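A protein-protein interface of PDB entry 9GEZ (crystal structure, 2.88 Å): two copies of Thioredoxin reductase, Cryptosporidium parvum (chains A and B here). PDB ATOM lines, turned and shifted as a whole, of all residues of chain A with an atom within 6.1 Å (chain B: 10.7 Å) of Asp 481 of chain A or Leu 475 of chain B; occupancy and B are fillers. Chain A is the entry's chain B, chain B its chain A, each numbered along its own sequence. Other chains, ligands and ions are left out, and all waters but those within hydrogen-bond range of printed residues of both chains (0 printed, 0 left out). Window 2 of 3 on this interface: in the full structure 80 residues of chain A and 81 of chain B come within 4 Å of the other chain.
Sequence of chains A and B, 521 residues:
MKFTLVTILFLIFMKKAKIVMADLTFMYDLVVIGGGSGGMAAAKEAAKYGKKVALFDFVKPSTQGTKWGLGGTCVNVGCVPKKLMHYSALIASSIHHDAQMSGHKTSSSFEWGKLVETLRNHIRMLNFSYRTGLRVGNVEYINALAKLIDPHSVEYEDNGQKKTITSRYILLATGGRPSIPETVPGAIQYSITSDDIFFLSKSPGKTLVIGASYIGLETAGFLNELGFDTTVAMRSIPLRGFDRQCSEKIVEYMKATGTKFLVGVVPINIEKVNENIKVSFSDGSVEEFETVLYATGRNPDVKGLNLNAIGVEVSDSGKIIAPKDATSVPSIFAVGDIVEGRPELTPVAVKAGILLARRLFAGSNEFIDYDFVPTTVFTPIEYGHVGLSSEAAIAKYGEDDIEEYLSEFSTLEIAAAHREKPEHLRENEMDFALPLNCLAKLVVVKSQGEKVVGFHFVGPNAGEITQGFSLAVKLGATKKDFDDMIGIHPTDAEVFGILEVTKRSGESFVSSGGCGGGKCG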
ATOM      1  N   ALA A 472       2.205 -26.955   7.070  1.00  0.00           N
ATOM      2  CA  ALA A 472       1.938 -25.572   6.631  1.00  0.00           C
ATOM      3  C   ALA A 472       1.835 -25.591   5.111  1.00  0.00           C
ATOM      4  O   ALA A 472       0.769 -25.180   4.558  1.00  0.00           O
ATOM      5  CB  ALA A 472       3.004 -24.645   7.119  1.00  0.00           C
ATOM      6  N   VAL A 473       2.856 -26.174   4.471  1.00  0.00           N
ATOM      7  CA  VAL A 473       2.862 -26.470   3.010  1.00  0.00           C
ATOM      8  C   VAL A 473       1.501 -27.074   2.682  1.00  0.00           C
ATOM      9  O   VAL A 473       0.758 -26.395   1.964  1.00  0.00           O
ATOM     10  CB  VAL A 473       4.031 -27.384   2.585  1.00  0.00           C
ATOM     11  CG1 VAL A 473       4.037 -27.650   1.080  1.00  0.00           C
ATOM     12  CG2 VAL A 473       5.377 -26.805   2.985  1.00  0.00           C
ATOM     13  N   LEU A 475      -1.300 -26.987   3.947  1.00  0.00           N
ATOM     14  CA  LEU A 475      -2.445 -26.049   4.126  1.00  0.00           C
ATOM     15  C   LEU A 475      -2.359 -24.913   3.098  1.00  0.00           C
ATOM     16  O   LEU A 475      -3.317 -24.092   3.048  1.00  0.00           O
ATOM     17  CB  LEU A 475      -2.521 -25.537   5.569  1.00  0.00           C
ATOM     18  CG  LEU A 475      -2.994 -26.566   6.596  1.00  0.00           C
ATOM     19  CD1 LEU A 475      -3.362 -25.914   7.920  1.00  0.00           C
ATOM     20  CD2 LEU A 475      -4.160 -27.378   6.068  1.00  0.00           C
ATOM     21  N   GLY A 476      -1.314 -24.916   2.263  1.00  0.00           N
ATOM     22  CA  GLY A 476      -1.182 -24.009   1.106  1.00  0.00           C
ATOM     23  C   GLY A 476      -0.451 -22.739   1.504  1.00  0.00           C
ATOM     24  O   GLY A 476      -0.928 -21.615   1.219  1.00  0.00           O
ATOM     25  N   ALA A 477       0.695 -22.912   2.157  1.00  0.00           N
ATOM     26  CA  ALA A 477       1.728 -21.870   2.304  1.00  0.00           C
ATOM     27  C   ALA A 477       2.183 -21.443   0.906  1.00  0.00           C
ATOM     28  O   ALA A 477       2.282 -22.309   0.004  1.00  0.00           O
ATOM     29  CB  ALA A 477       2.882 -22.371   3.142  1.00  0.00           C
ATOM     30  N   THR A 478       2.386 -20.136   0.757  1.00  0.00           N
ATOM     31  CA  THR A 478       2.968 -19.456  -0.420  1.00  0.00           C
ATOM     32  C   THR A 478       4.291 -18.863   0.013  1.00  0.00           C
ATOM     33  O   THR A 478       4.472 -18.716   1.242  1.00  0.00           O
ATOM     34  CB  THR A 478       2.106 -18.279  -0.895  1.00  0.00           C
ATOM     35  OG1 THR A 478       2.064 -17.353   0.190  1.00  0.00           O
ATOM     36  CG2 THR A 478       0.721 -18.696  -1.334  1.00  0.00           C
ATOM     37  N   LYS A 479       5.135 -18.466  -0.938  1.00  0.00           N
ATOM     38  CA  LYS A 479       6.391 -17.747  -0.612  1.00  0.00           C
ATOM     39  C   LYS A 479       6.056 -16.511   0.233  1.00  0.00           C
ATOM     40  O   LYS A 479       6.833 -16.230   1.152  1.00  0.00           O
ATOM     41  CB  LYS A 479       7.158 -17.372  -1.877  1.00  0.00           C
ATOM     42  CG  LYS A 479       8.479 -16.673  -1.623  1.00  0.00           C
ATOM     43  CD  LYS A 479       9.416 -17.478  -0.742  1.00  0.00           C
ATOM     44  CE  LYS A 479      10.860 -17.037  -0.822  1.00  0.00           C
ATOM     45  NZ  LYS A 479      11.002 -15.561  -0.886  1.00  0.00           N
ATOM     46  N   LYS A 480       4.936 -15.832  -0.029  1.00  0.00           N
ATOM     47  CA  LYS A 480       4.616 -14.584   0.715  1.00  0.00           C
ATOM     48  C   LYS A 480       4.332 -14.920   2.180  1.00  0.00           C
ATOM     49  O   LYS A 480       4.838 -14.189   3.003  1.00  0.00           O
ATOM     50  CB  LYS A 480       3.419 -13.803   0.170  1.00  0.00           C
ATOM     51  CG  LYS A 480       3.370 -12.372   0.684  1.00  0.00           C
ATOM     52  CD  LYS A 480       1.997 -11.863   1.089  1.00  0.00           C
ATOM     53  CE  LYS A 480       2.067 -10.805   2.174  1.00  0.00           C
ATOM     54  NZ  LYS A 480       3.245  -9.909   2.024  1.00  0.00           N
ATOM     55  N   ASP A 481       3.540 -15.963   2.466  1.00  0.00           N
ATOM     56  CA  ASP A 481       3.261 -16.483   3.835  1.00  0.00           C
ATOM     57  C   ASP A 481       4.583 -16.791   4.558  1.00  0.00           C
ATOM     58  O   ASP A 481       4.731 -16.417   5.760  1.00  0.00           O
ATOM     59  CB  ASP A 481       2.474 -17.792   3.804  1.00  0.00           C
ATOM     60  CG  ASP A 481       1.038 -17.661   3.355  1.00  0.00           C
ATOM     61  OD1 ASP A 481       0.317 -16.839   3.943  1.00  0.00           O
ATOM     62  OD2 ASP A 481       0.660 -18.401   2.439  1.00  0.00           O
ATOM     63  N   PHE A 482       5.525 -17.422   3.848  1.00  0.00           N
ATOM     64  CA  PHE A 482       6.854 -17.792   4.393  1.00  0.00           C
ATOM     65  C   PHE A 482       7.641 -16.543   4.754  1.00  0.00           C
ATOM     66  O   PHE A 482       8.201 -16.591   5.824  1.00  0.00           O
ATOM     67  CB  PHE A 482       7.650 -18.641   3.407  1.00  0.00           C
ATOM     68  CG  PHE A 482       7.424 -20.123   3.577  1.00  0.00           C
ATOM     69  CD1 PHE A 482       7.922 -20.789   4.672  1.00  0.00           C
ATOM     70  CD2 PHE A 482       6.672 -20.843   2.656  1.00  0.00           C
ATOM     71  CE1 PHE A 482       7.725 -22.149   4.819  1.00  0.00           C
ATOM     72  CE2 PHE A 482       6.474 -22.207   2.807  1.00  0.00           C
ATOM     73  CZ  PHE A 482       7.022 -22.859   3.881  1.00  0.00           C
ATOM     74  N   ASP A 483       7.674 -15.508   3.911  1.00  0.00           N
ATOM     75  CA  ASP A 483       8.503 -14.287   4.125  1.00  0.00           C
ATOM     76  C   ASP A 483       7.894 -13.377   5.194  1.00  0.00           C
ATOM     77  O   ASP A 483       8.619 -12.508   5.673  1.00  0.00           O
ATOM     78  CB  ASP A 483       8.643 -13.449   2.855  1.00  0.00           C
ATOM     79  CG  ASP A 483       9.285 -14.206   1.713  1.00  0.00           C
ATOM     80  OD1 ASP A 483       9.446 -15.430   1.854  1.00  0.00           O
ATOM     81  OD2 ASP A 483       9.621 -13.559   0.699  1.00  0.00           O
ATOM     82  N   ASP A 484       6.593 -13.528   5.475  1.00  0.00           N
ATOM     83  CA  ASP A 484       5.839 -12.802   6.529  1.00  0.00           C
ATOM     84  C   ASP A 484       5.902 -13.581   7.844  1.00  0.00           C
ATOM     85  O   ASP A 484       5.477 -13.017   8.862  1.00  0.00           O
ATOM     86  CB  ASP A 484       4.375 -12.638   6.120  1.00  0.00           C
ATOM     87  CG  ASP A 484       4.151 -11.557   5.085  1.00  0.00           C
ATOM     88  OD1 ASP A 484       4.837 -11.612   4.029  1.00  0.00           O
ATOM     89  OD2 ASP A 484       3.289 -10.684   5.336  1.00  0.00           O
ATOM     90  N   MET A 485       6.332 -14.848   7.794  1.00  0.00           N
ATOM     91  CA  MET A 485       6.694 -15.689   8.972  1.00  0.00           C
ATOM     92  C   MET A 485       7.697 -14.907   9.817  1.00  0.00           C
ATOM     93  O   MET A 485       8.710 -14.431   9.224  1.00  0.00           O
ATOM     94  CB  MET A 485       7.343 -17.007   8.535  1.00  0.00           C
ATOM     95  CG  MET A 485       7.350 -18.110   9.571  1.00  0.00           C
ATOM     96  SD  MET A 485       8.317 -19.597   9.045  1.00  0.00           S
ATOM     97  CE  MET A 485       9.905 -18.838   8.742  1.00  0.00           C
ATOM     98  N   LYS B 351      12.106  -7.847  11.274  1.00  0.00           N
ATOM     99  CA  LYS B 351      10.885  -7.686  10.430  1.00  0.00           C
ATOM    100  C   LYS B 351      10.399  -6.240  10.504  1.00  0.00           C
ATOM    101  O   LYS B 351      10.114  -5.659   9.463  1.00  0.00           O
ATOM    102  CB  LYS B 351       9.676  -8.513  10.878  1.00  0.00           C
ATOM    103  CG  LYS B 351       9.787 -10.024  10.773  1.00  0.00           C
ATOM    104  CD  LYS B 351      10.584 -10.522   9.594  1.00  0.00           C
ATOM    105  CE  LYS B 351      10.021 -10.118   8.245  1.00  0.00           C
ATOM    106  NZ  LYS B 351      11.117 -10.040   7.251  1.00  0.00           N
ATOM    107  N   ARG B 358      10.966  -0.458   4.056  1.00  0.00           N
ATOM    108  CA  ARG B 358      10.111  -0.654   2.851  1.00  0.00           C
ATOM    109  C   ARG B 358       8.998   0.410   2.806  1.00  0.00           C
ATOM    110  O   ARG B 358       8.869   1.083   1.782  1.00  0.00           O
ATOM    111  CB  ARG B 358       9.472  -2.043   2.825  1.00  0.00           C
ATOM    112  CG  ARG B 358      10.344  -3.122   2.207  1.00  0.00           C
ATOM    113  CD  ARG B 358       9.639  -4.462   2.231  1.00  0.00           C
ATOM    114  NE  ARG B 358      10.591  -5.556   2.318  1.00  0.00           N
ATOM    115  CZ  ARG B 358      10.282  -6.834   2.535  1.00  0.00           C
ATOM    116  NH1 ARG B 358       9.022  -7.207   2.702  1.00  0.00           N
ATOM    117  NH2 ARG B 358      11.251  -7.732   2.601  1.00  0.00           N
ATOM    118  N   GLU B 366       2.794  -2.745   4.812  1.00  0.00           N
ATOM    119  CA  GLU B 366       2.830  -3.987   5.624  1.00  0.00           C
ATOM    120  C   GLU B 366       3.300  -3.622   7.037  1.00  0.00           C
ATOM    121  O   GLU B 366       4.181  -2.729   7.173  1.00  0.00           O
ATOM    122  CB  GLU B 366       3.750  -5.031   4.980  1.00  0.00           C
ATOM    123  CG  GLU B 366       3.597  -5.145   3.465  1.00  0.00           C
ATOM    124  CD  GLU B 366       3.901  -6.517   2.885  1.00  0.00           C
ATOM    125  OE1 GLU B 366       3.835  -7.507   3.653  1.00  0.00           O
ATOM    126  OE2 GLU B 366       4.187  -6.599   1.678  1.00  0.00           O
ATOM    127  N   ASP B 369       2.011  -8.846  11.906  1.00  0.00           N
ATOM    128  CA  ASP B 369       0.970  -9.616  12.636  1.00  0.00           C
ATOM    129  C   ASP B 369       1.596 -10.017  13.986  1.00  0.00           C
ATOM    130  O   ASP B 369       2.452 -10.994  14.019  1.00  0.00           O
ATOM    131  CB  ASP B 369       0.509 -10.795  11.777  1.00  0.00           C
ATOM    132  CG  ASP B 369      -0.852 -11.351  12.152  1.00  0.00           C
ATOM    133  OD1 ASP B 369      -1.201 -11.313  13.404  1.00  0.00           O
ATOM    134  OD2 ASP B 369      -1.545 -11.846  11.210  1.00  0.00           O
ATOM    135  N   ASP B 371      -0.024 -11.062  16.496  1.00  0.00           N
ATOM    136  CA  ASP B 371      -0.790 -12.200  17.075  1.00  0.00           C
ATOM    137  C   ASP B 371       0.016 -13.506  16.951  1.00  0.00           C
ATOM    138  O   ASP B 371      -0.393 -14.473  17.545  1.00  0.00           O
ATOM    139  CB  ASP B 371      -2.189 -12.298  16.462  1.00  0.00           C
ATOM    140  CG  ASP B 371      -3.081 -11.131  16.868  1.00  0.00           C
ATOM    141  OD1 ASP B 371      -2.812 -10.554  17.951  1.00  0.00           O
ATOM    142  OD2 ASP B 371      -4.039 -10.802  16.103  1.00  0.00           O
ATOM    143  N   PHE B 372       1.128 -13.516  16.218  1.00  0.00           N
ATOM    144  CA  PHE B 372       1.867 -14.758  15.834  1.00  0.00           C
ATOM    145  C   PHE B 372       3.379 -14.481  15.839  1.00  0.00           C
ATOM    146  O   PHE B 372       4.033 -14.289  14.772  1.00  0.00           O
ATOM    147  CB  PHE B 372       1.389 -15.307  14.485  1.00  0.00           C
ATOM    148  CG  PHE B 372      -0.073 -15.677  14.473  1.00  0.00           C
ATOM    149  CD1 PHE B 372      -0.500 -16.854  15.066  1.00  0.00           C
ATOM    150  CD2 PHE B 372      -1.024 -14.834  13.917  1.00  0.00           C
ATOM    151  CE1 PHE B 372      -1.840 -17.196  15.074  1.00  0.00           C
ATOM    152  CE2 PHE B 372      -2.370 -15.173  13.938  1.00  0.00           C
ATOM    153  CZ  PHE B 372      -2.772 -16.354  14.513  1.00  0.00           C
ATOM    154  N   PRO B 374       6.507 -16.459  17.395  1.00  0.00           N
ATOM    155  CA  PRO B 374       7.031 -17.626  18.095  1.00  0.00           C
ATOM    156  C   PRO B 374       8.152 -17.101  18.998  1.00  0.00           C
ATOM    157  O   PRO B 374       8.570 -15.961  18.768  1.00  0.00           O
ATOM    158  CB  PRO B 374       7.524 -18.534  16.966  1.00  0.00           C
ATOM    159  CG  PRO B 374       7.939 -17.534  15.955  1.00  0.00           C
ATOM    160  CD  PRO B 374       6.842 -16.489  15.964  1.00  0.00           C
ATOM    161  N   VAL B 386       3.820 -20.622  20.032  1.00  0.00           N
ATOM    162  CA  VAL B 386       3.123 -19.430  19.449  1.00  0.00           C
ATOM    163  C   VAL B 386       1.684 -19.366  19.947  1.00  0.00           C
ATOM    164  O   VAL B 386       1.093 -20.400  20.289  1.00  0.00           O
ATOM    165  CB  VAL B 386       3.139 -19.395  17.911  1.00  0.00           C
ATOM    166  CG1 VAL B 386       2.369 -20.532  17.277  1.00  0.00           C
ATOM    167  CG2 VAL B 386       2.636 -18.059  17.399  1.00  0.00           C
ATOM    168  N   LYS B 451     -10.312 -24.757  16.128  1.00  0.00           N
ATOM    169  CA  LYS B 451      -9.230 -23.896  15.563  1.00  0.00           C
ATOM    170  C   LYS B 451      -8.112 -23.771  16.602  1.00  0.00           C
ATOM    171  O   LYS B 451      -8.426 -23.618  17.790  1.00  0.00           O
ATOM    172  CB  LYS B 451      -9.750 -22.510  15.176  1.00  0.00           C
ATOM    173  CG  LYS B 451      -8.721 -21.541  14.604  1.00  0.00           C
ATOM    174  CD  LYS B 451      -9.288 -20.161  14.375  1.00  0.00           C
ATOM    175  CE  LYS B 451      -8.484 -19.034  14.992  1.00  0.00           C
ATOM    176  NZ  LYS B 451      -7.480 -18.492  14.045  1.00  0.00           N
ATOM    177  N   VAL B 452      -6.855 -23.807  16.156  1.00  0.00           N
ATOM    178  CA  VAL B 452      -5.679 -23.870  17.064  1.00  0.00           C
ATOM    179  C   VAL B 452      -5.171 -22.447  17.383  1.00  0.00           C
ATOM    180  O   VAL B 452      -4.768 -21.721  16.460  1.00  0.00           O
ATOM    181  CB  VAL B 452      -4.608 -24.778  16.463  1.00  0.00           C
ATOM    182  CG1 VAL B 452      -3.558 -25.138  17.494  1.00  0.00           C
ATOM    183  CG2 VAL B 452      -5.231 -26.035  15.882  1.00  0.00           C
ATOM    184  N   VAL B 453      -5.228 -22.088  18.675  1.00  0.00           N
ATOM    185  CA  VAL B 453      -4.947 -20.737  19.251  1.00  0.00           C
ATOM    186  C   VAL B 453      -3.707 -20.809  20.154  1.00  0.00           C
ATOM    187  O   VAL B 453      -3.167 -19.719  20.406  1.00  0.00           O
ATOM    188  CB  VAL B 453      -6.167 -20.163  20.011  1.00  0.00           C
ATOM    189  CG1 VAL B 453      -7.474 -20.417  19.258  1.00  0.00           C
ATOM    190  CG2 VAL B 453      -6.286 -20.676  21.442  1.00  0.00           C
ATOM    191  N   GLN B 467       8.973 -23.842  14.906  1.00  0.00           N
ATOM    192  CA  GLN B 467       9.021 -22.903  13.730  1.00  0.00           C
ATOM    193  C   GLN B 467       7.979 -23.327  12.691  1.00  0.00           C
ATOM    194  O   GLN B 467       6.919 -22.664  12.595  1.00  0.00           O
ATOM    195  CB  GLN B 467      10.406 -22.781  13.092  1.00  0.00           C
ATOM    196  CG  GLN B 467      10.444 -21.767  11.954  1.00  0.00           C
ATOM    197  CD  GLN B 467      10.648 -20.334  12.411  1.00  0.00           C
ATOM    198  OE1 GLN B 467      11.765 -19.962  12.752  1.00  0.00           O
ATOM    199  NE2 GLN B 467       9.607 -19.499  12.348  1.00  0.00           N
ATOM    200  N   GLY B 468       8.243 -24.417  11.980  1.00  0.00           N
ATOM    201  CA  GLY B 468       7.276 -24.988  11.020  1.00  0.00           C
ATOM    202  C   GLY B 468       5.845 -24.878  11.542  1.00  0.00           C
ATOM    203  O   GLY B 468       5.026 -24.245  10.836  1.00  0.00           O
ATOM    204  N   PHE B 469       5.566 -25.345  12.774  1.00  0.00           N
ATOM    205  CA  PHE B 469       4.207 -25.306  13.370  1.00  0.00           C
ATOM    206  C   PHE B 469       3.729 -23.869  13.630  1.00  0.00           C
ATOM    207  O   PHE B 469       2.500 -23.672  13.495  1.00  0.00           O
ATOM    208  CB  PHE B 469       4.148 -26.175  14.627  1.00  0.00           C
ATOM    209  CG  PHE B 469       3.945 -27.646  14.337  1.00  0.00           C
ATOM    210  CD1 PHE B 469       2.806 -28.082  13.698  1.00  0.00           C
ATOM    211  CD2 PHE B 469       4.893 -28.589  14.686  1.00  0.00           C
ATOM    212  CE1 PHE B 469       2.614 -29.415  13.388  1.00  0.00           C
ATOM    213  CE2 PHE B 469       4.697 -29.934  14.404  1.00  0.00           C
ATOM    214  CZ  PHE B 469       3.569 -30.339  13.738  1.00  0.00           C
ATOM    215  N   SER B 470       4.583 -22.885  13.947  1.00  0.00           N
ATOM    216  CA  SER B 470       4.108 -21.467  14.015  1.00  0.00           C
ATOM    217  C   SER B 470       3.355 -21.109  12.715  1.00  0.00           C
ATOM    218  O   SER B 470       2.140 -20.666  12.802  1.00  0.00           O
ATOM    219  CB  SER B 470       5.195 -20.463  14.312  1.00  0.00           C
ATOM    220  OG  SER B 470       6.048 -20.192  13.184  1.00  0.00           O
ATOM    221  N   LEU B 471       3.938 -21.383  11.534  1.00  0.00           N
ATOM    222  CA  LEU B 471       3.270 -21.001  10.252  1.00  0.00           C
ATOM    223  C   LEU B 471       1.975 -21.785  10.015  1.00  0.00           C
ATOM    224  O   LEU B 471       1.073 -21.162   9.430  1.00  0.00           O
ATOM    225  CB  LEU B 471       4.195 -21.177   9.049  1.00  0.00           C
ATOM    226  CG  LEU B 471       3.481 -21.008   7.709  1.00  0.00           C
ATOM    227  CD1 LEU B 471       2.914 -19.605   7.578  1.00  0.00           C
ATOM    228  CD2 LEU B 471       4.415 -21.310   6.538  1.00  0.00           C
ATOM    229  N   ALA B 472       1.860 -23.068  10.388  1.00  0.00           N
ATOM    230  CA  ALA B 472       0.588 -23.815  10.164  1.00  0.00           C
ATOM    231  C   ALA B 472      -0.530 -23.130  10.959  1.00  0.00           C
ATOM    232  O   ALA B 472      -1.514 -22.684  10.347  1.00  0.00           O
ATOM    233  CB  ALA B 472       0.696 -25.278  10.524  1.00  0.00           C
ATOM    234  N   VAL B 473      -0.325 -22.952  12.266  1.00  0.00           N
ATOM    235  CA  VAL B 473      -1.166 -22.080  13.148  1.00  0.00           C
ATOM    236  C   VAL B 473      -1.523 -20.806  12.353  1.00  0.00           C
ATOM    237  O   VAL B 473      -2.673 -20.640  12.019  1.00  0.00           O
ATOM    238  CB  VAL B 473      -0.417 -21.763  14.463  1.00  0.00           C
ATOM    239  CG1 VAL B 473      -1.103 -20.672  15.293  1.00  0.00           C
ATOM    240  CG2 VAL B 473      -0.200 -23.013  15.311  1.00  0.00           C
ATOM    241  N   LYS B 474      -0.532 -19.982  11.983  1.00  0.00           N
ATOM    242  CA  LYS B 474      -0.774 -18.658  11.329  1.00  0.00           C
ATOM    243  C   LYS B 474      -1.549 -18.862  10.008  1.00  0.00           C
ATOM    244  O   LYS B 474      -2.172 -17.879   9.567  1.00  0.00           O
ATOM    245  CB  LYS B 474       0.528 -17.863  11.107  1.00  0.00           C
ATOM    246  CG  LYS B 474       0.345 -16.407  10.641  1.00  0.00           C
ATOM    247  CD  LYS B 474       1.577 -15.771  10.002  1.00  0.00           C
ATOM    248  CE  LYS B 474       1.607 -14.255  10.059  1.00  0.00           C
ATOM    249  NZ  LYS B 474       2.835 -13.670   9.440  1.00  0.00           N
ATOM    250  N   LEU B 475      -1.506 -20.050   9.374  1.00  0.00           N
ATOM    251  CA  LEU B 475      -2.325 -20.328   8.150  1.00  0.00           C
ATOM    252  C   LEU B 475      -3.716 -20.843   8.563  1.00  0.00           C
ATOM    253  O   LEU B 475      -4.508 -21.167   7.636  1.00  0.00           O
ATOM    254  CB  LEU B 475      -1.639 -21.332   7.210  1.00  0.00           C
ATOM    255  CG  LEU B 475      -0.373 -20.874   6.472  1.00  0.00           C
ATOM    256  CD1 LEU B 475      -0.121 -21.743   5.245  1.00  0.00           C
ATOM    257  CD2 LEU B 475      -0.419 -19.410   6.057  1.00  0.00           C
ATOM    258  N   GLY B 476      -3.998 -20.938   9.876  1.00  0.00           N
ATOM    259  CA  GLY B 476      -5.334 -21.197  10.447  1.00  0.00           C
ATOM    260  C   GLY B 476      -5.623 -22.685  10.586  1.00  0.00           C
ATOM    261  O   GLY B 476      -6.733 -23.108  10.178  1.00  0.00           O
ATOM    262  N   ALA B 477      -4.661 -23.460  11.096  1.00  0.00           N
ATOM    263  CA  ALA B 477      -4.790 -24.923  11.302  1.00  0.00           C
ATOM    264  C   ALA B 477      -5.888 -25.200  12.325  1.00  0.00           C
ATOM    265  O   ALA B 477      -6.075 -24.379  13.245  1.00  0.00           O
ATOM    266  CB  ALA B 477      -3.478 -25.527  11.767  1.00  0.00           C
ATOM    267  N   THR B 478      -6.538 -26.349  12.154  1.00  0.00           N
ATOM    268  CA  THR B 478      -7.439 -27.027  13.125  1.00  0.00           C
ATOM    269  C   THR B 478      -6.805 -28.336  13.625  1.00  0.00           C
ATOM    270  O   THR B 478      -5.867 -28.883  12.949  1.00  0.00           O
ATOM    271  CB  THR B 478      -8.744 -27.445  12.444  1.00  0.00           C
ATOM    272  OG1 THR B 478      -8.365 -28.379  11.432  1.00  0.00           O
ATOM    273  CG2 THR B 478      -9.511 -26.308  11.813  1.00  0.00           C
ATOM    274  N   ASP B 481      -6.783 -30.960  10.796  1.00  0.00           N
ATOM    275  CA  ASP B 481      -5.584 -30.847   9.929  1.00  0.00           C
ATOM    276  C   ASP B 481      -4.390 -31.526  10.598  1.00  0.00           C
ATOM    277  O   ASP B 481      -3.636 -32.234   9.900  1.00  0.00           O
ATOM    278  CB  ASP B 481      -5.308 -29.373   9.658  1.00  0.00           C
ATOM    279  CG  ASP B 481      -6.531 -28.659   9.100  1.00  0.00           C
ATOM    280  OD1 ASP B 481      -7.182 -29.203   8.161  1.00  0.00           O
ATOM    281  OD2 ASP B 481      -6.854 -27.588   9.636  1.00  0.00           O
ATOM    282  N   PHE B 482      -4.246 -31.334  11.914  1.00  0.00           N
ATOM    283  CA  PHE B 482      -3.174 -31.939  12.751  1.00  0.00           C
ATOM    284  C   PHE B 482      -3.247 -33.460  12.669  1.00  0.00           C
ATOM    285  O   PHE B 482      -2.195 -34.032  12.474  1.00  0.00           O
ATOM    286  CB  PHE B 482      -3.272 -31.500  14.211  1.00  0.00           C
ATOM    287  CG  PHE B 482      -2.422 -30.319  14.582  1.00  0.00           C
ATOM    288  CD1 PHE B 482      -2.637 -29.081  14.008  1.00  0.00           C
ATOM    289  CD2 PHE B 482      -1.396 -30.457  15.506  1.00  0.00           C
ATOM    290  CE1 PHE B 482      -1.845 -27.998  14.347  1.00  0.00           C
ATOM    291  CE2 PHE B 482      -0.578 -29.381  15.814  1.00  0.00           C
ATOM    292  CZ  PHE B 482      -0.812 -28.151  15.239  1.00  0.00           C
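Of chain B, only Leu 475 comes within 4 Å of Asp 481 of chain A. Leu 475 of chain B touches just these residues of chain A: Ala 472 (3.6 Å), Gly 476 (3.9 Å), Ala 477 (3.4 Å) and Asp 481 (3.4 Å). Ala 472 of chain A touches just these residues of chain B: Leu 471, Ala 472 and Leu 475. Of chain B, only Leu 471 and Leu 475 come within 4 Å of Ala 477 of chain A. Of chain B, only Leu 471 (3.8 Å) comes within 4 Å of Phe 482 of chain A. Of the printed residues of chain A, Gln 467 of chain B touches Met 485. Printed residues of chain A within 4 Å of Leu 471 of chain B: Ala 472, Ala 477 and Phe 482. Printed residues of chain A within 4 Å of Ala 472 of chain B: Ala 472 (3.8 Å). Of the printed residues of chain A, Lys 474 of chain B touches Asp 484 (2.8 Å). Printed residues of chain A within 4 Å of Lys 351 of chain B: Asp 483 (3.8 Å). Gly 476 of chain B touches none of the printed residues of chain A. The nearest residue of chain A that does not touch Leu 475 of chain B is Leu 475 of chain A (4.4 Å).
The side-chain amino group of Lys 480 of chain A is in salt-bridge range of the side-chain carboxylate of Glu 366 of chain B. NE2 of Gln 467 of chain B lies within hydrogen-bond range of SD of Met 485 of chain A (3.5 Å). The backbone carbonyl oxygen (O) of Asp 484 of chain A is in hydrogen-bond range of the side-chain amino group (NZ) of Lys 474 of chain B (2.8 Å).
Leu 475 of chain A touches Ala 477 of chain B, and with the chains exchanged Ala 477 of chain A touches Leu 475 of chain B. Gly 476 of chain A touches Leu 475 of chain B, but with the chains exchanged Leu 475 of chain A does not touch Gly 476 of chain B (4.8 Å). Asp 481 of chain A touches Leu 475 of chain B, but with the chains exchanged Leu 475 of chain A does not touch Asp 481 of chain B (4.1 Å). Positions printed for both chains: 472, 473, 475, 476, 477, 478, 481 and 482.
Among the printed residues, merely in contact across the chains: Ala 477 of chain A with Leu 475 of chain B (3.4 Å), Asp 481 of chain A with Leu 475 of chain B (3.4 Å), Ala 472 of chain A with Leu 475 of chain B (3.6 Å), Asp 484 of chain A with Glu 366 of chain B (3.6 Å), Ala 472 of chain A with Leu 471 of chain B (3.7 Å), Asp 483 of chain A with Lys 351 of chain B (3.8 Å), Leu 475 of chain A with Ala 477 of chain B (3.8 Å), Ala 472 of chain A with Ala 472 of chain B (3.8 Å), Phe 482 of chain A with Leu 471 of chain B (3.8 Å), Ala 477 of chain A with Leu 471 of chain B (3.9 Å) and Gly 476 of chain A with Leu 475 of chain B (3.9 Å).
Hydrophobic or aromatic side chains of chain A within 4 Å of the printed part of chain B: Ala 472, Leu 475, Ala 477, Phe 482 and Met 485. Hydrophobic or aromatic side chains of chain B that line the printed part of chain A: Leu 471, Leu 475 and Ala 477. Among the printed residues, Asp or Glu carboxylates within 4 Å of a Lys or Arg side-chain nitrogen of the other chain: Lys 480 of chain A with Glu 366 of chain B (3.0 Å).
The backbone NH (N) of Val 452 of chain B sits at hydrogen-bond distance from the backbone carbonyl oxygen (O) of Ala 477 of chain B, at 3.1 Å. The side-chain hydroxyl of Ser 470 of chain B sits at hydrogen-bond distance from the backbone carbonyl oxygen of Gln 467 of chain B (2.7 Å). The backbone NH of Lys 480 of chain A lies close to the side-chain hydroxyl of Thr 478 of chain A.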
